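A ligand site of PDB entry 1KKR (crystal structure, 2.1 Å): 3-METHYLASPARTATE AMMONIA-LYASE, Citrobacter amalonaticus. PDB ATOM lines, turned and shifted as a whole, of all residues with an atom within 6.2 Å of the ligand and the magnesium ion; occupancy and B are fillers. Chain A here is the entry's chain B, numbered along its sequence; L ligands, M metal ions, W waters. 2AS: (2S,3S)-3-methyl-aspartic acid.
O of the ligand lies within hydrogen-bond range of SG of Cys 361. An oxygen (OD1) of the ligand sits close to the side-chain amide nitrogen (NE2) of Gln 329, at 3.1 Å. OE1 of Gln 172 is in hydrogen-bond range of N of the ligand (2.8 Å). The backbone NH of Cys 361 sits at hydrogen-bond distance from an oxygen (O) of the ligand (2.8 Å). The side-chain hydroxyl (OG1) of Thr 360 is in hydrogen-bond range of an oxygen (OXT) of the ligand, at 2.7 Å. The side-chain amino group of Lys 331 lies close to an oxygen (OD1) of the ligand (3.4 Å). A ring nitrogen (NE2) of His 194 is in hydrogen-bond range of an oxygen (OD2) of the ligand, 2.9 Å away. OD2 of the ligand lies within hydrogen-bond range of OH of Tyr 240 (3.4 Å).
The side-chain carboxylate of Asp 307 lies within salt-bridge range of the side-chain amino group of Lys 331, at 3.1 Å. The side-chain carboxylate of Glu 273 sits close to the side-chain amide nitrogen of Gln 329 (2.9 Å). N of Tyr 240 sits at hydrogen-bond distance from OD1 of Asp 238, at 3.1 Å. A ring nitrogen (ND1) of His 194 sits at hydrogen-bond distance from the backbone NH of Leu 196 (3.0 Å). The side-chain amide nitrogen (NE2) of Gln 329 lies close to the side-chain carboxylate (OD2) of Asp 307, 3.3 Å away. N of Asp 238 is in hydrogen-bond range of O of His 194, 3.0 Å away. The side-chain hydroxyl of Thr 360 sits at hydrogen-bond distance from the backbone NH of Asn 362 (3.0 Å). The side-chain amide oxygen (OE1) of Gln 329 is in hydrogen-bond range of the backbone NH (N) of Gly 359, 3.1 Å away.
Gly 359 touches the ligand. Leu 384 touches the ligand. Hydrophobic or aromatic side chains that line the ligand: His 194, Tyr 240 and Leu 384. Within 4 Å of the ligand: Gln 172, His 194, Asp 238, Tyr 240, Glu 273, Asp 307, Gln 329, Lys 331, Gly 359, Thr 360, Cys 361 and Leu 384.
Glu 308 touches the magnesium ion. NE2 of Gln 329 touches the magnesium ion (3.8 Å). Five residues have an atom within 4 Å of the magnesium ion: Asp 238, Glu 273, Asp 307, Glu 308 and Gln 329. The nearest printed residue that does not touch the magnesium ion is Lys 331 (4.04 Å).
The magnesium ion is bound by water W1, the side-chain carboxylate of Asp 307, the side-chain carboxylate of Asp 238, water W6, the side-chain carboxylate of Glu 273 and an oxygen (OD1) of the ligand.
Water W1 bridges the side-chain carboxylate of Glu 308 (2.6 Å) and an oxygen (OD2) of the ligand (3.0 Å). Water W6 lies within hydrogen-bond range of OE2 of Glu 308 (2.8 Å) and OD1 of Asp 238 (2.9 Å). Water W2 bridges an oxygen (OXT) of the ligand (2.6 Å) and the side-chain amino group of Lys 331 (3.0 Å). Water W4 lies within hydrogen-bond range of N of the ligand, OH of Tyr 240 and OE1 of Gln 73. Water W5 lies within hydrogen-bond range of OH of Tyr 356, OE1 of Glu 273 and NE2 of Gln 329. Water W3 lies within hydrogen-bond range of the side-chain hydroxyl of Tyr 240 (2.5 Å) and an oxygen (OD2) of the ligand (3.5 Å).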
ATOM      1  N   VAL A  72       1.374  21.091   4.853  1.00  0.00           N
ATOM      2  CA  VAL A  72       1.342  22.005   3.737  1.00  0.00           C
ATOM      3  C   VAL A  72      -0.070  22.418   3.328  1.00  0.00           C
ATOM      4  O   VAL A  72      -1.056  21.852   3.797  1.00  0.00           O
ATOM      5  CB  VAL A  72       2.042  21.387   2.550  1.00  0.00           C
ATOM      6  CG1 VAL A  72       3.471  21.058   2.939  1.00  0.00           C
ATOM      7  CG2 VAL A  72       1.229  20.133   2.029  1.00  0.00           C
ATOM      8  N   GLN A  73      -0.140  23.428   2.460  1.00  0.00           N
ATOM      9  CA  GLN A  73      -1.406  23.978   1.949  1.00  0.00           C
ATOM     10  C   GLN A  73      -2.277  22.949   1.191  1.00  0.00           C
ATOM     11  O   GLN A  73      -3.483  22.879   1.373  1.00  0.00           O
ATOM     12  CB  GLN A  73      -1.107  25.214   1.041  1.00  0.00           C
ATOM     13  CG  GLN A  73      -2.375  25.778   0.367  1.00  0.00           C
ATOM     14  CD  GLN A  73      -2.125  26.945  -0.660  1.00  0.00           C
ATOM     15  OE1 GLN A  73      -1.032  27.493  -0.753  1.00  0.00           O
ATOM     16  NE2 GLN A  73      -3.172  27.291  -1.409  1.00  0.00           N
ATOM     17  N   GLN A 172       8.643  34.843  -0.016  1.00  0.00           N
ATOM     18  CA  GLN A 172       7.659  34.383  -0.966  1.00  0.00           C
ATOM     19  C   GLN A 172       6.504  35.359  -0.974  1.00  0.00           C
ATOM     20  O   GLN A 172       6.035  35.826   0.049  1.00  0.00           O
ATOM     21  CB  GLN A 172       7.260  32.945  -0.728  1.00  0.00           C
ATOM     22  CG  GLN A 172       6.207  32.715   0.318  1.00  0.00           C
ATOM     23  CD  GLN A 172       5.695  31.286   0.302  1.00  0.00           C
ATOM     24  OE1 GLN A 172       5.403  30.721  -0.768  1.00  0.00           O
ATOM     25  NE2 GLN A 172       5.579  30.678   1.479  1.00  0.00           N
ATOM     26  N   HIS A 194       9.857  34.458  -5.154  1.00  0.00           N
ATOM     27  CA  HIS A 194       9.007  33.292  -5.424  1.00  0.00           C
ATOM     28  C   HIS A 194       8.027  33.526  -6.592  1.00  0.00           C
ATOM     29  O   HIS A 194       8.100  32.832  -7.594  1.00  0.00           O
ATOM     30  CB  HIS A 194       8.309  32.744  -4.163  1.00  0.00           C
ATOM     31  CG  HIS A 194       7.591  31.461  -4.418  1.00  0.00           C
ATOM     32  ND1 HIS A 194       6.378  31.406  -5.081  1.00  0.00           N
ATOM     33  CD2 HIS A 194       7.892  30.178  -4.087  1.00  0.00           C
ATOM     34  CE1 HIS A 194       5.979  30.148  -5.148  1.00  0.00           C
ATOM     35  NE2 HIS A 194       6.868  29.392  -4.544  1.00  0.00           N
ATOM     36  N   LEU A 196       4.992  32.905  -7.254  1.00  0.00           N
ATOM     37  CA  LEU A 196       3.880  32.026  -7.526  1.00  0.00           C
ATOM     38  C   LEU A 196       3.498  32.052  -9.033  1.00  0.00           C
ATOM     39  O   LEU A 196       2.360  32.377  -9.380  1.00  0.00           O
ATOM     40  CB  LEU A 196       2.660  32.468  -6.685  1.00  0.00           C
ATOM     41  CG  LEU A 196       1.552  31.440  -6.489  1.00  0.00           C
ATOM     42  CD1 LEU A 196       2.120  30.165  -5.872  1.00  0.00           C
ATOM     43  CD2 LEU A 196       0.380  31.950  -5.642  1.00  0.00           C
ATOM     44  N   ASP A 238       9.450  30.314  -8.616  1.00  0.00           N
ATOM     45  CA  ASP A 238       8.888  28.974  -8.655  1.00  0.00           C
ATOM     46  C   ASP A 238       7.813  29.014  -9.731  1.00  0.00           C
ATOM     47  O   ASP A 238       6.892  29.834  -9.689  1.00  0.00           O
ATOM     48  CB  ASP A 238       8.286  28.675  -7.263  1.00  0.00           C
ATOM     49  CG  ASP A 238       7.821  27.278  -7.079  1.00  0.00           C
ATOM     50  OD1 ASP A 238       7.547  26.564  -8.064  1.00  0.00           O
ATOM     51  OD2 ASP A 238       7.695  26.801  -5.926  1.00  0.00           O
ATOM     52  N   TYR A 240       6.115  26.206 -10.739  1.00  0.00           N
ATOM     53  CA  TYR A 240       5.213  25.078 -10.500  1.00  0.00           C
ATOM     54  C   TYR A 240       4.945  24.225 -11.739  1.00  0.00           C
ATOM     55  O   TYR A 240       3.796  24.000 -12.114  1.00  0.00           O
ATOM     56  CB  TYR A 240       3.866  25.579 -10.001  1.00  0.00           C
ATOM     57  CG  TYR A 240       3.633  25.853  -8.536  1.00  0.00           C
ATOM     58  CD1 TYR A 240       4.214  26.980  -7.861  1.00  0.00           C
ATOM     59  CD2 TYR A 240       2.745  25.056  -7.843  1.00  0.00           C
ATOM     60  CE1 TYR A 240       3.931  27.232  -6.456  1.00  0.00           C
ATOM     61  CE2 TYR A 240       2.425  25.297  -6.500  1.00  0.00           C
ATOM     62  CZ  TYR A 240       2.993  26.380  -5.789  1.00  0.00           C
ATOM     63  OH  TYR A 240       2.594  26.528  -4.440  1.00  0.00           O
ATOM     64  N   GLU A 273      12.628  27.449  -9.773  1.00  0.00           N
ATOM     65  CA  GLU A 273      12.229  26.298  -9.015  1.00  0.00           C
ATOM     66  C   GLU A 273      11.103  25.560  -9.685  1.00  0.00           C
ATOM     67  O   GLU A 273      10.199  26.173 -10.165  1.00  0.00           O
ATOM     68  CB  GLU A 273      11.748  26.725  -7.601  1.00  0.00           C
ATOM     69  CG  GLU A 273      11.149  25.588  -6.741  1.00  0.00           C
ATOM     70  CD  GLU A 273      10.818  25.991  -5.282  1.00  0.00           C
ATOM     71  OE1 GLU A 273      11.350  26.987  -4.720  1.00  0.00           O
ATOM     72  OE2 GLU A 273       9.980  25.302  -4.680  1.00  0.00           O
ATOM     73  N   GLY A 274      11.122  24.236  -9.607  1.00  0.00           N
ATOM     74  CA  GLY A 274      10.045  23.413 -10.127  1.00  0.00           C
ATOM     75  C   GLY A 274       9.789  23.578 -11.634  1.00  0.00           C
ATOM     76  O   GLY A 274       8.684  23.892 -12.002  1.00  0.00           O
ATOM     77  N   ASP A 307      11.464  20.452  -6.209  1.00  0.00           N
ATOM     78  CA  ASP A 307      10.510  20.569  -5.118  1.00  0.00           C
ATOM     79  C   ASP A 307       9.566  19.346  -5.132  1.00  0.00           C
ATOM     80  O   ASP A 307       9.742  18.373  -4.375  1.00  0.00           O
ATOM     81  CB  ASP A 307       9.724  21.877  -5.257  1.00  0.00           C
ATOM     82  CG  ASP A 307       8.786  22.145  -4.096  1.00  0.00           C
ATOM     83  OD1 ASP A 307       8.797  21.372  -3.115  1.00  0.00           O
ATOM     84  OD2 ASP A 307       8.002  23.121  -4.073  1.00  0.00           O
ATOM     85  N   GLU A 308       8.655  19.374  -6.083  1.00  0.00           N
ATOM     86  CA  GLU A 308       7.642  18.358  -6.201  1.00  0.00           C
ATOM     87  C   GLU A 308       8.381  17.022  -6.393  1.00  0.00           C
ATOM     88  O   GLU A 308       9.398  16.967  -7.072  1.00  0.00           O
ATOM     89  CB  GLU A 308       6.682  18.685  -7.369  1.00  0.00           C
ATOM     90  CG  GLU A 308       5.717  19.830  -7.106  1.00  0.00           C
ATOM     91  CD  GLU A 308       6.340  21.224  -6.964  1.00  0.00           C
ATOM     92  OE1 GLU A 308       5.657  22.085  -6.387  1.00  0.00           O
ATOM     93  OE2 GLU A 308       7.482  21.461  -7.417  1.00  0.00           O
ATOM     94  N   GLN A 329      14.579  21.682  -2.595  1.00  0.00           N
ATOM     95  CA  GLN A 329      13.755  22.144  -1.485  1.00  0.00           C
ATOM     96  C   GLN A 329      13.473  21.033  -0.520  1.00  0.00           C
ATOM     97  O   GLN A 329      12.764  20.130  -0.845  1.00  0.00           O
ATOM     98  CB  GLN A 329      12.394  22.723  -1.861  1.00  0.00           C
ATOM     99  CG  GLN A 329      11.865  23.508  -0.571  1.00  0.00           C
ATOM    100  CD  GLN A 329      10.526  24.162  -0.653  1.00  0.00           C
ATOM    101  OE1 GLN A 329       9.863  24.374   0.424  1.00  0.00           O
ATOM    102  NE2 GLN A 329      10.096  24.513  -1.880  1.00  0.00           N
ATOM    103  N   LYS A 331      11.324  20.467   2.040  1.00  0.00           N
ATOM    104  CA  LYS A 331      10.058  21.106   2.420  1.00  0.00           C
ATOM    105  C   LYS A 331       9.748  20.606   3.826  1.00  0.00           C
ATOM    106  O   LYS A 331       9.161  19.550   3.972  1.00  0.00           O
ATOM    107  CB  LYS A 331       8.944  20.794   1.423  1.00  0.00           C
ATOM    108  CG  LYS A 331       7.655  21.676   1.624  1.00  0.00           C
ATOM    109  CD  LYS A 331       6.738  21.587   0.403  1.00  0.00           C
ATOM    110  CE  LYS A 331       7.210  22.564  -0.714  1.00  0.00           C
ATOM    111  NZ  LYS A 331       6.330  22.760  -1.930  1.00  0.00           N
ATOM    112  N   TYR A 356      18.098  23.884   0.331  1.00  0.00           N
ATOM    113  CA  TYR A 356      17.130  24.967   0.547  1.00  0.00           C
ATOM    114  C   TYR A 356      16.146  24.468   1.590  1.00  0.00           C
ATOM    115  O   TYR A 356      15.304  23.587   1.321  1.00  0.00           O
ATOM    116  CB  TYR A 356      16.413  25.376  -0.757  1.00  0.00           C
ATOM    117  CG  TYR A 356      15.067  26.079  -0.676  1.00  0.00           C
ATOM    118  CD1 TYR A 356      14.758  26.915   0.356  1.00  0.00           C
ATOM    119  CD2 TYR A 356      14.099  25.913  -1.695  1.00  0.00           C
ATOM    120  CE1 TYR A 356      13.541  27.551   0.412  1.00  0.00           C
ATOM    121  CE2 TYR A 356      12.848  26.568  -1.652  1.00  0.00           C
ATOM    122  CZ  TYR A 356      12.578  27.357  -0.567  1.00  0.00           C
ATOM    123  OH  TYR A 356      11.403  28.007  -0.412  1.00  0.00           O
ATOM    124  N   GLY A 359       9.633  24.942   3.488  1.00  0.00           N
ATOM    125  CA  GLY A 359       8.500  24.776   4.378  1.00  0.00           C
ATOM    126  C   GLY A 359       7.245  25.236   3.681  1.00  0.00           C
ATOM    127  O   GLY A 359       7.148  25.173   2.457  1.00  0.00           O
ATOM    128  N   THR A 360       6.275  25.717   4.446  1.00  0.00           N
ATOM    129  CA  THR A 360       5.076  26.227   3.846  1.00  0.00           C
ATOM    130  C   THR A 360       4.508  27.482   4.468  1.00  0.00           C
ATOM    131  O   THR A 360       4.765  27.762   5.647  1.00  0.00           O
ATOM    132  CB  THR A 360       4.069  25.121   3.888  1.00  0.00           C
ATOM    133  OG1 THR A 360       2.828  25.570   3.385  1.00  0.00           O
ATOM    134  CG2 THR A 360       3.707  24.710   5.301  1.00  0.00           C
ATOM    135  N   CYS A 361       3.749  28.256   3.688  1.00  0.00           N
ATOM    136  CA  CYS A 361       2.977  29.378   4.259  1.00  0.00           C
ATOM    137  C   CYS A 361       2.000  28.851   5.313  1.00  0.00           C
ATOM    138  O   CYS A 361       1.596  29.569   6.236  1.00  0.00           O
ATOM    139  CB  CYS A 361       2.136  30.131   3.187  1.00  0.00           C
ATOM    140  SG  CYS A 361       0.946  29.094   2.287  1.00  0.00           S
ATOM    141  N   ASN A 362       1.618  27.588   5.221  1.00  0.00           N
ATOM    142  CA  ASN A 362       0.557  27.080   6.120  1.00  0.00           C
ATOM    143  C   ASN A 362       1.030  26.479   7.440  1.00  0.00           C
ATOM    144  O   ASN A 362       0.269  25.717   8.063  1.00  0.00           O
ATOM    145  CB  ASN A 362      -0.269  26.038   5.387  1.00  0.00           C
ATOM    146  CG  ASN A 362      -1.617  25.794   6.032  1.00  0.00           C
ATOM    147  OD1 ASN A 362      -2.352  26.713   6.362  1.00  0.00           O
ATOM    148  ND2 ASN A 362      -1.959  24.523   6.183  1.00  0.00           N
ATOM    149  N   LEU A 384      13.513  29.309   3.975  1.00  0.00           N
ATOM    150  CA  LEU A 384      12.274  29.991   3.679  1.00  0.00           C
ATOM    151  C   LEU A 384      11.757  30.933   4.826  1.00  0.00           C
ATOM    152  O   LEU A 384      11.714  30.535   5.963  1.00  0.00           O
ATOM    153  CB  LEU A 384      11.207  28.957   3.287  1.00  0.00           C
ATOM    154  CG  LEU A 384       9.793  29.513   3.055  1.00  0.00           C
ATOM    155  CD1 LEU A 384       9.765  30.378   1.835  1.00  0.00           C
ATOM    156  CD2 LEU A 384       8.748  28.442   2.837  1.00  0.00           C
ATOM    157  N   MET A 389       1.500  34.413   4.175  1.00  0.00           N
ATOM    158  CA  MET A 389       1.666  35.027   2.867  1.00  0.00           C
ATOM    159  C   MET A 389       1.765  36.530   2.986  1.00  0.00           C
ATOM    160  O   MET A 389       1.748  37.219   1.988  1.00  0.00           O
ATOM    161  CB  MET A 389       0.478  34.639   1.976  1.00  0.00           C
ATOM    162  CG  MET A 389       0.539  33.169   1.446  1.00  0.00           C
ATOM    163  SD  MET A 389       2.191  32.845   0.445  1.00  0.00           S
ATOM    164  CE  MET A 389       2.096  34.009  -0.034  1.00  0.00           C
HETATM  165  C   2AS L   1       3.974  26.922   0.285  1.00  0.00           C
HETATM  166  O   2AS L   1       3.907  27.998   0.876  1.00  0.00           O
HETATM  167  CA  2AS L   1       4.454  26.935  -1.153  1.00  0.00           C
HETATM  168  N   2AS L   1       4.375  28.309  -1.695  1.00  0.00           N
HETATM  169  CB  2AS L   1       5.910  26.479  -1.199  1.00  0.00           C
HETATM  170  CG  2AS L   1       6.435  26.367  -2.618  1.00  0.00           C
HETATM  171  OD1 2AS L   1       7.483  25.776  -2.857  1.00  0.00           O
HETATM  172  C4  2AS L   1       6.870  27.422  -0.466  1.00  0.00           C
HETATM  173  OD2 2AS L   1       5.824  26.924  -3.512  1.00  0.00           O
HETATM  174  OXT 2AS L   1       3.645  25.883   0.833  1.00  0.00           O
HETATM  175 MG    MG M   1       7.851  24.995  -4.928  1.00  0.00          MG
HETATM  176  O   HOH W   1       5.895  24.455  -5.258  1.00  0.00           O
HETATM  177  O   HOH W   2       3.790  23.776  -0.756  1.00  0.00           O
HETATM  178  O   HOH W   3       3.563  24.304  -3.655  1.00  0.00           O
HETATM  179  O   HOH W   4       1.700  28.549  -2.386  1.00  0.00           O
HETATM  180  O   HOH W   5       9.841  27.608  -2.540  1.00  0.00           O
HETATM  181  O   HOH W   6       8.220  24.043  -6.787  1.00  0.00           O
HETATM  182  O   HOH W   7       1.552  24.349   0.307  1.00  0.00           O
